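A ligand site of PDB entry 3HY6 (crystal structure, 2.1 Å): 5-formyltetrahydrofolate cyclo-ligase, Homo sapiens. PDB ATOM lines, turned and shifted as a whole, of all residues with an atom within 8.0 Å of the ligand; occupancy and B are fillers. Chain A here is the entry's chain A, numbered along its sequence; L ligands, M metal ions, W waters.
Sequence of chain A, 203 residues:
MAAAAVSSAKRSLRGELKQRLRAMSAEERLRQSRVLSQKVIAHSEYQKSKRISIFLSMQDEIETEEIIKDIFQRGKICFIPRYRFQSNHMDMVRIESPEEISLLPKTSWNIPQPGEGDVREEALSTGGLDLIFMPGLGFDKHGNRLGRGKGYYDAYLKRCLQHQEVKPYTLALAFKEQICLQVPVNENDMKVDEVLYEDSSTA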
ATOM      1  N   VAL A   6     -16.634 -17.329 -12.167  1.00  0.00           N
ATOM      2  CA  VAL A   6     -16.122 -18.509 -12.901  1.00  0.00           C
ATOM      3  C   VAL A   6     -16.684 -19.824 -12.318  1.00  0.00           C
ATOM      4  O   VAL A   6     -17.199 -20.657 -13.069  1.00  0.00           O
ATOM      5  CB  VAL A   6     -14.566 -18.569 -12.910  1.00  0.00           C
ATOM      6  CG1 VAL A   6     -14.074 -19.856 -13.578  1.00  0.00           C
ATOM      7  CG2 VAL A   6     -13.989 -17.372 -13.663  1.00  0.00           C
ATOM      8  N   SER A   7     -16.617 -19.983 -10.996  1.00  0.00           N
ATOM      9  CA  SER A   7     -17.145 -21.208 -10.353  1.00  0.00           C
ATOM     10  C   SER A   7     -18.613 -21.393 -10.624  1.00  0.00           C
ATOM     11  O   SER A   7     -19.079 -22.506 -10.780  1.00  0.00           O
ATOM     12  CB  SER A   7     -16.935 -21.201  -8.836  1.00  0.00           C
ATOM     13  OG  SER A   7     -15.605 -20.875  -8.507  1.00  0.00           O
ATOM     14  N   LYS A  10     -19.140 -22.629 -14.156  1.00  0.00           N
ATOM     15  CA  LYS A  10     -18.690 -24.023 -14.232  1.00  0.00           C
ATOM     16  C   LYS A  10     -19.756 -24.921 -13.632  1.00  0.00           C
ATOM     17  O   LYS A  10     -20.103 -25.952 -14.215  1.00  0.00           O
ATOM     18  CB  LYS A  10     -17.373 -24.226 -13.464  1.00  0.00           C
ATOM     19  CG  LYS A  10     -16.114 -23.672 -14.103  1.00  0.00           C
ATOM     20  CD  LYS A  10     -14.899 -23.951 -13.200  1.00  0.00           C
ATOM     21  CE  LYS A  10     -13.602 -23.584 -13.911  1.00  0.00           C
ATOM     22  NZ  LYS A  10     -12.413 -23.940 -13.097  1.00  0.00           N
ATOM     23  N   ARG A  11     -20.268 -24.515 -12.459  1.00  0.00           N
ATOM     24  CA  ARG A  11     -21.331 -25.239 -11.768  1.00  0.00           C
ATOM     25  C   ARG A  11     -22.605 -25.343 -12.628  1.00  0.00           C
ATOM     26  O   ARG A  11     -23.195 -26.413 -12.748  1.00  0.00           O
ATOM     27  CB  ARG A  11     -21.608 -24.594 -10.401  1.00  0.00           C
ATOM     28  CG  ARG A  11     -22.910 -25.045  -9.725  1.00  0.00           C
ATOM     29  CD  ARG A  11     -23.243 -24.197  -8.482  1.00  0.00           C
ATOM     30  NE  ARG A  11     -23.330 -22.758  -8.780  1.00  0.00           N
ATOM     31  CZ  ARG A  11     -24.404 -22.151  -9.299  1.00  0.00           C
ATOM     32  NH1 ARG A  11     -25.508 -22.846  -9.591  1.00  0.00           N
ATOM     33  NH2 ARG A  11     -24.387 -20.852  -9.524  1.00  0.00           N
ATOM     34  N   ARG A  14     -21.970 -27.742 -15.494  1.00  0.00           N
ATOM     35  CA  ARG A  14     -21.983 -29.134 -15.020  1.00  0.00           C
ATOM     36  C   ARG A  14     -23.397 -29.719 -14.916  1.00  0.00           C
ATOM     37  O   ARG A  14     -23.652 -30.853 -15.349  1.00  0.00           O
ATOM     38  CB  ARG A  14     -21.285 -29.279 -13.678  1.00  0.00           C
ATOM     39  CG  ARG A  14     -19.761 -29.192 -13.764  1.00  0.00           C
ATOM     40  CD  ARG A  14     -19.091 -29.437 -12.412  1.00  0.00           C
ATOM     41  NE  ARG A  14     -17.699 -29.021 -12.463  1.00  0.00           N
ATOM     42  CZ  ARG A  14     -17.181 -27.981 -11.814  1.00  0.00           C
ATOM     43  NH1 ARG A  14     -17.936 -27.239 -11.002  1.00  0.00           N
ATOM     44  NH2 ARG A  14     -15.898 -27.693 -11.970  1.00  0.00           N
ATOM     45  N   ASN A  88      -7.665 -33.176  -3.253  1.00  0.00           N
ATOM     46  CA  ASN A  88      -7.613 -33.256  -4.709  1.00  0.00           C
ATOM     47  C   ASN A  88      -6.369 -34.052  -5.171  1.00  0.00           C
ATOM     48  O   ASN A  88      -5.745 -33.705  -6.203  1.00  0.00           O
ATOM     49  CB  ASN A  88      -7.600 -31.852  -5.353  1.00  0.00           C
ATOM     50  CG  ASN A  88      -6.362 -31.044  -4.964  1.00  0.00           C
ATOM     51  OD1 ASN A  88      -5.693 -31.327  -3.953  1.00  0.00           O
ATOM     52  ND2 ASN A  88      -6.049 -30.011  -5.761  1.00  0.00           N
ATOM     53  N   GLY A 136     -13.978 -36.256 -18.223  1.00  0.00           N
ATOM     54  CA  GLY A 136     -14.475 -34.947 -17.860  1.00  0.00           C
ATOM     55  C   GLY A 136     -15.945 -34.865 -18.197  1.00  0.00           C
ATOM     56  O   GLY A 136     -16.480 -35.702 -18.939  1.00  0.00           O
ATOM     57  N   LEU A 137     -16.592 -33.849 -17.637  1.00  0.00           N
ATOM     58  CA  LEU A 137     -18.007 -33.611 -17.923  1.00  0.00           C
ATOM     59  C   LEU A 137     -18.182 -32.892 -19.250  1.00  0.00           C
ATOM     60  O   LEU A 137     -19.103 -33.203 -20.012  1.00  0.00           O
ATOM     61  CB  LEU A 137     -18.654 -32.824 -16.786  1.00  0.00           C
ATOM     62  CG  LEU A 137     -18.946 -33.579 -15.504  1.00  0.00           C
ATOM     63  CD1 LEU A 137     -19.647 -32.619 -14.549  1.00  0.00           C
ATOM     64  CD2 LEU A 137     -19.815 -34.785 -15.794  1.00  0.00           C
ATOM     65  N   GLY A 138     -17.304 -31.937 -19.532  1.00  0.00           N
ATOM     66  CA  GLY A 138     -17.358 -31.222 -20.811  1.00  0.00           C
ATOM     67  C   GLY A 138     -16.027 -30.734 -21.362  1.00  0.00           C
ATOM     68  O   GLY A 138     -15.065 -30.475 -20.616  1.00  0.00           O
ATOM     69  N   ARG A 145     -11.176 -28.095 -20.568  1.00  0.00           N
ATOM     70  CA  ARG A 145     -11.874 -29.216 -19.928  1.00  0.00           C
ATOM     71  C   ARG A 145     -12.661 -28.771 -18.715  1.00  0.00           C
ATOM     72  O   ARG A 145     -12.198 -27.920 -17.925  1.00  0.00           O
ATOM     73  CB  ARG A 145     -10.894 -30.326 -19.512  1.00  0.00           C
ATOM     74  CG  ARG A 145     -11.604 -31.603 -19.047  1.00  0.00           C
ATOM     75  CD  ARG A 145     -10.642 -32.707 -18.644  1.00  0.00           C
ATOM     76  NE  ARG A 145      -9.930 -32.273 -17.464  1.00  0.00           N
ATOM     77  CZ  ARG A 145     -10.206 -32.644 -16.222  1.00  0.00           C
ATOM     78  NH1 ARG A 145     -11.117 -33.556 -15.959  1.00  0.00           N
ATOM     79  NH2 ARG A 145      -9.506 -32.099 -15.255  1.00  0.00           N
ATOM     80  N   LEU A 146     -13.842 -29.375 -18.563  1.00  0.00           N
ATOM     81  CA  LEU A 146     -14.648 -29.170 -17.375  1.00  0.00           C
ATOM     82  C   LEU A 146     -14.717 -30.495 -16.642  1.00  0.00           C
ATOM     83  O   LEU A 146     -15.318 -31.442 -17.145  1.00  0.00           O
ATOM     84  CB  LEU A 146     -16.040 -28.649 -17.743  1.00  0.00           C
ATOM     85  CG  LEU A 146     -17.059 -28.514 -16.588  1.00  0.00           C
ATOM     86  CD1 LEU A 146     -16.553 -27.635 -15.426  1.00  0.00           C
ATOM     87  CD2 LEU A 146     -18.366 -27.992 -17.097  1.00  0.00           C
ATOM     88  N   GLY A 147     -14.063 -30.568 -15.482  1.00  0.00           N
ATOM     89  CA  GLY A 147     -14.118 -31.757 -14.631  1.00  0.00           C
ATOM     90  C   GLY A 147     -15.325 -31.787 -13.696  1.00  0.00           C
ATOM     91  O   GLY A 147     -16.308 -31.069 -13.917  1.00  0.00           O
ATOM     92  N   ARG A 148     -15.252 -32.589 -12.645  1.00  0.00           N
ATOM     93  CA  ARG A 148     -16.380 -32.765 -11.700  1.00  0.00           C
ATOM     94  C   ARG A 148     -16.350 -31.781 -10.520  1.00  0.00           C
ATOM     95  O   ARG A 148     -17.260 -31.773  -9.683  1.00  0.00           O
ATOM     96  CB  ARG A 148     -16.462 -34.204 -11.213  1.00  0.00           C
ATOM     97  CG  ARG A 148     -16.734 -35.163 -12.327  1.00  0.00           C
ATOM     98  CD  ARG A 148     -16.685 -36.623 -11.920  1.00  0.00           C
ATOM     99  NE  ARG A 148     -16.864 -37.497 -13.084  1.00  0.00           N
ATOM    100  CZ  ARG A 148     -18.046 -37.860 -13.586  1.00  0.00           C
ATOM    101  NH1 ARG A 148     -19.174 -37.438 -13.036  1.00  0.00           N
ATOM    102  NH2 ARG A 148     -18.100 -38.645 -14.653  1.00  0.00           N
ATOM    103  N   GLY A 149     -15.311 -30.966 -10.443  1.00  0.00           N
ATOM    104  CA  GLY A 149     -15.245 -29.962  -9.415  1.00  0.00           C
ATOM    105  C   GLY A 149     -14.075 -30.129  -8.460  1.00  0.00           C
ATOM    106  O   GLY A 149     -13.786 -29.225  -7.688  1.00  0.00           O
ATOM    107  N   LYS A 150     -13.413 -31.268  -8.503  1.00  0.00           N
ATOM    108  CA  LYS A 150     -12.359 -31.524  -7.519  1.00  0.00           C
ATOM    109  C   LYS A 150     -10.978 -31.097  -7.987  1.00  0.00           C
ATOM    110  O   LYS A 150     -10.073 -30.914  -7.159  1.00  0.00           O
ATOM    111  CB  LYS A 150     -12.343 -33.001  -7.117  1.00  0.00           C
ATOM    112  CG  LYS A 150     -13.501 -33.379  -6.224  1.00  0.00           C
ATOM    113  CD  LYS A 150     -13.293 -32.859  -4.790  1.00  0.00           C
ATOM    114  CE  LYS A 150     -14.612 -32.410  -4.171  1.00  0.00           C
ATOM    115  NZ  LYS A 150     -14.994 -31.037  -4.638  1.00  0.00           N
ATOM    116  N   GLY A 151     -10.814 -30.957  -9.304  1.00  0.00           N
ATOM    117  CA  GLY A 151      -9.531 -30.583  -9.894  1.00  0.00           C
ATOM    118  C   GLY A 151      -8.403 -31.606  -9.758  1.00  0.00           C
ATOM    119  O   GLY A 151      -7.240 -31.233  -9.786  1.00  0.00           O
ATOM    120  N   TYR A 152      -8.766 -32.872  -9.593  1.00  0.00           N
ATOM    121  CA  TYR A 152      -7.804 -33.984  -9.523  1.00  0.00           C
ATOM    122  C   TYR A 152      -6.887 -34.049 -10.749  1.00  0.00           C
ATOM    123  O   TYR A 152      -5.669 -34.117 -10.621  1.00  0.00           O
ATOM    124  CB  TYR A 152      -8.567 -35.321  -9.472  1.00  0.00           C
ATOM    125  CG  TYR A 152      -9.141 -35.721  -8.131  1.00  0.00           C
ATOM    126  CD1 TYR A 152     -10.520 -35.837  -7.942  1.00  0.00           C
ATOM    127  CD2 TYR A 152      -8.302 -36.027  -7.060  1.00  0.00           C
ATOM    128  CE1 TYR A 152     -11.051 -36.236  -6.696  1.00  0.00           C
ATOM    129  CE2 TYR A 152      -8.815 -36.442  -5.830  1.00  0.00           C
ATOM    130  CZ  TYR A 152     -10.183 -36.514  -5.648  1.00  0.00           C
ATOM    131  OH  TYR A 152     -10.668 -36.903  -4.441  1.00  0.00           O
ATOM    132  N   TYR A 153      -7.503 -34.050 -11.932  1.00  0.00           N
ATOM    133  CA  TYR A 153      -6.750 -34.113 -13.190  1.00  0.00           C
ATOM    134  C   TYR A 153      -5.919 -32.880 -13.535  1.00  0.00           C
ATOM    135  O   TYR A 153      -4.805 -33.039 -14.044  1.00  0.00           O
ATOM    136  CB  TYR A 153      -7.666 -34.512 -14.363  1.00  0.00           C
ATOM    137  CG  TYR A 153      -7.755 -35.999 -14.542  1.00  0.00           C
ATOM    138  CD1 TYR A 153      -8.777 -36.733 -13.925  1.00  0.00           C
ATOM    139  CD2 TYR A 153      -6.813 -36.679 -15.289  1.00  0.00           C
ATOM    140  CE1 TYR A 153      -8.867 -38.119 -14.098  1.00  0.00           C
ATOM    141  CE2 TYR A 153      -6.888 -38.070 -15.463  1.00  0.00           C
ATOM    142  CZ  TYR A 153      -7.910 -38.774 -14.853  1.00  0.00           C
ATOM    143  OH  TYR A 153      -7.988 -40.146 -15.013  1.00  0.00           O
ATOM    144  N   ASP A 154      -6.433 -31.678 -13.262  1.00  0.00           N
ATOM    145  CA  ASP A 154      -5.614 -30.470 -13.344  1.00  0.00           C
ATOM    146  C   ASP A 154      -4.366 -30.619 -12.466  1.00  0.00           C
ATOM    147  O   ASP A 154      -3.251 -30.397 -12.935  1.00  0.00           O
ATOM    148  CB  ASP A 154      -6.376 -29.213 -12.898  1.00  0.00           C
ATOM    149  CG  ASP A 154      -7.622 -28.932 -13.721  1.00  0.00           C
ATOM    150  OD1 ASP A 154      -7.585 -29.037 -14.970  1.00  0.00           O
ATOM    151  OD2 ASP A 154      -8.630 -28.565 -13.094  1.00  0.00           O
ATOM    152  N   ALA A 155      -4.541 -30.976 -11.189  1.00  0.00           N
ATOM    153  CA  ALA A 155      -3.407 -31.120 -10.260  1.00  0.00           C
ATOM    154  C   ALA A 155      -2.418 -32.191 -10.702  1.00  0.00           C
ATOM    155  O   ALA A 155      -1.203 -31.982 -10.640  1.00  0.00           O
ATOM    156  CB  ALA A 155      -3.887 -31.396  -8.827  1.00  0.00           C
ATOM    157  N   VAL A 183     -16.118 -23.549 -22.667  1.00  0.00           N
ATOM    158  CA  VAL A 183     -15.962 -24.077 -21.305  1.00  0.00           C
ATOM    159  C   VAL A 183     -15.327 -22.981 -20.466  1.00  0.00           C
ATOM    160  O   VAL A 183     -14.270 -22.446 -20.828  1.00  0.00           O
ATOM    161  CB  VAL A 183     -15.131 -25.394 -21.295  1.00  0.00           C
ATOM    162  CG1 VAL A 183     -14.692 -25.754 -19.883  1.00  0.00           C
ATOM    163  CG2 VAL A 183     -15.930 -26.529 -21.909  1.00  0.00           C
ATOM    164  N   PRO A 184     -15.979 -22.617 -19.339  1.00  0.00           N
ATOM    165  CA  PRO A 184     -15.409 -21.598 -18.438  1.00  0.00           C
ATOM    166  C   PRO A 184     -14.156 -22.144 -17.769  1.00  0.00           C
ATOM    167  O   PRO A 184     -14.173 -23.260 -17.255  1.00  0.00           O
ATOM    168  CB  PRO A 184     -16.528 -21.373 -17.391  1.00  0.00           C
ATOM    169  CG  PRO A 184     -17.734 -22.049 -17.924  1.00  0.00           C
ATOM    170  CD  PRO A 184     -17.240 -23.160 -18.807  1.00  0.00           C
ATOM    171  N   VAL A 185     -13.080 -21.371 -17.802  1.00  0.00           N
ATOM    172  CA  VAL A 185     -11.806 -21.777 -17.192  1.00  0.00           C
ATOM    173  C   VAL A 185     -11.154 -20.646 -16.412  1.00  0.00           C
ATOM    174  O   VAL A 185     -11.444 -19.470 -16.643  1.00  0.00           O
ATOM    175  CB  VAL A 185     -10.787 -22.324 -18.258  1.00  0.00           C
ATOM    176  CG1 VAL A 185     -11.259 -23.640 -18.844  1.00  0.00           C
ATOM    177  CG2 VAL A 185     -10.525 -21.290 -19.363  1.00  0.00           C
ATOM    178  N   ASN A 186     -10.286 -20.986 -15.456  1.00  0.00           N
ATOM    179  CA  ASN A 186      -9.361 -19.995 -14.870  1.00  0.00           C
ATOM    180  C   ASN A 186      -7.902 -20.332 -15.203  1.00  0.00           C
ATOM    181  O   ASN A 186      -7.635 -21.270 -15.950  1.00  0.00           O
ATOM    182  CB  ASN A 186      -9.563 -19.817 -13.362  1.00  0.00           C
ATOM    183  CG  ASN A 186      -9.660 -21.138 -12.613  1.00  0.00           C
ATOM    184  OD1 ASN A 186     -10.756 -21.570 -12.249  1.00  0.00           O
ATOM    185  ND2 ASN A 186      -8.533 -21.782 -12.374  1.00  0.00           N
ATOM    186  N   ASN A 188      -5.783 -21.721 -13.509  1.00  0.00           N
ATOM    187  CA  ASN A 188      -5.391 -23.000 -12.909  1.00  0.00           C
ATOM    188  C   ASN A 188      -5.779 -24.244 -13.714  1.00  0.00           C
ATOM    189  O   ASN A 188      -5.209 -25.314 -13.503  1.00  0.00           O
ATOM    190  N   ASP A 189      -6.739 -24.090 -14.626  1.00  0.00           N
ATOM    191  CA  ASP A 189      -7.266 -25.202 -15.430  1.00  0.00           C
ATOM    192  C   ASP A 189      -6.297 -25.616 -16.551  1.00  0.00           C
ATOM    193  O   ASP A 189      -5.658 -24.765 -17.163  1.00  0.00           O
ATOM    194  CB  ASP A 189      -8.644 -24.840 -16.018  1.00  0.00           C
ATOM    195  CG  ASP A 189      -9.711 -24.644 -14.946  1.00  0.00           C
ATOM    196  OD1 ASP A 189      -9.857 -25.536 -14.084  1.00  0.00           O
ATOM    197  OD2 ASP A 189     -10.398 -23.602 -14.957  1.00  0.00           O
ATOM    198  N   MET A 190      -6.226 -26.912 -16.820  1.00  0.00           N
ATOM    199  CA  MET A 190      -5.242 -27.457 -17.756  1.00  0.00           C
ATOM    200  C   MET A 190      -5.893 -27.937 -19.053  1.00  0.00           C
ATOM    201  O   MET A 190      -6.759 -28.806 -19.021  1.00  0.00           O
ATOM    202  CB  MET A 190      -4.494 -28.623 -17.096  1.00  0.00           C
ATOM    203  CG  MET A 190      -3.748 -28.274 -15.812  1.00  0.00           C
ATOM    204  SD  MET A 190      -2.374 -27.122 -16.060  1.00  0.00           S
ATOM    205  CE  MET A 190      -1.198 -28.188 -16.912  1.00  0.00           C
HETATM  206  P1  LIG L   1     -12.692 -29.370 -12.172  1.00  0.00           P
HETATM  207  O1  LIG L   1     -14.012 -29.156 -13.138  1.00  0.00           O
HETATM  208  O2  LIG L   1     -12.628 -30.900 -11.581  1.00  0.00           O
HETATM  209  O3  LIG L   1     -11.452 -29.087 -12.934  1.00  0.00           O
HETATM  210  P2  LIG L   1     -11.970 -26.986 -10.719  1.00  0.00           P
HETATM  211  O4  LIG L   1     -10.950 -26.760 -11.998  1.00  0.00           O
HETATM  212  O5  LIG L   1     -13.046 -25.748 -10.542  1.00  0.00           O
HETATM  213  O6  LIG L   1     -12.888 -28.326 -10.920  1.00  0.00           O
HETATM  214  O7  LIG L   1     -11.188 -27.152  -9.482  1.00  0.00           O
HETATM  215 MG    MG M   1     -10.426 -27.990 -15.263  1.00  0.00          MG
HETATM  216  O   HOH W   1     -12.815 -27.002 -14.219  1.00  0.00           O
HETATM  217  O   HOH W   2     -14.694 -24.592  -8.878  1.00  0.00           O
HETATM  218  O   HOH W   3      -8.073 -27.406 -10.704  1.00  0.00           O
HETATM  219  O   HOH W   4      -9.193 -24.424 -11.787  1.00  0.00           O
HETATM  220  O   HOH W   5     -13.285 -22.342 -10.740  1.00  0.00           O
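O2 of the ligand is in hydrogen-bond range of N of Gly 149. An oxygen (O4) of the ligand sits close to the side-chain carboxylate (OD1) of Asp 189. The backbone NH (N) of Gly 151 is in hydrogen-bond range of an oxygen (O2) of the ligand. An oxygen (O3) of the ligand lies close to the side-chain carboxylate of Asp 154, at 2.9 Å. NZ of Lys 10 lies within salt-bridge range of O5 of the ligand (3.2 Å). An oxygen (O1) of the ligand sits at hydrogen-bond distance from the backbone NH of Gly 147 (2.7 Å). An oxygen (O2) of the ligand lies within hydrogen-bond range of the backbone NH (N) of Lys 150, at 3.2 Å. NH2 of Arg 14 lies within salt-bridge range of O1 of the ligand, at 2.7 Å. The backbone carbonyl oxygen of Gly 147 lies close to an oxygen (O1) of the ligand. N of Arg 148 is in hydrogen-bond range of O2 of the ligand (3.3 Å).
The side-chain amino group (NZ) of Lys 10 is in salt-bridge range of the side-chain carboxylate (OD2) of Asp 189, at 2.8 Å. The side-chain carboxylate of Asp 189 lies within hydrogen-bond range of the backbone NH of Asn 186. The side-chain amide oxygen (OD1) of Asn 186 is in hydrogen-bond range of the side-chain amino group (NZ) of Lys 10. The guanidinium group of Arg 14 is in hydrogen-bond range of the backbone carbonyl oxygen of Gly 147 (2.9 Å). N of Leu 137 is in hydrogen-bond range of O of Leu 146 (2.8 Å). N of Met 190 is in hydrogen-bond range of OD1 of Asp 154 (3.1 Å). The side-chain carboxylate (OD1) of Asp 154 is in salt-bridge range of the guanidinium group (NH2) of Arg 145, 3.6 Å away. N of Leu 146 lies within hydrogen-bond range of O of Gly 138, 2.6 Å away.
Leu 146 touches the ligand. Hydrophobic or aromatic side chains within 4 Å of the ligand: Leu 146. The nearest printed residue that does not touch the ligand is Arg 145 (4.3 Å).
Water W1 lies within hydrogen-bond range of O1 of the ligand (2.7 Å), NZ of Lys 10 (3.3 Å) and OD1 of Asp 189 (3.3 Å). Water W4 lies within hydrogen-bond range of OD1 of Asp 189, ND2 of Asn 186 and O4 of the ligand. Water W3 lies within hydrogen-bond range of OD2 of Asp 154 (2.7 Å) and O4 of the ligand (3.2 Å). Water W5 lies within hydrogen-bond range of the side-chain amino group (NZ) of Lys 10, the side-chain amide oxygen (OD1) of Asn 186 and an oxygen (O5) of the ligand.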
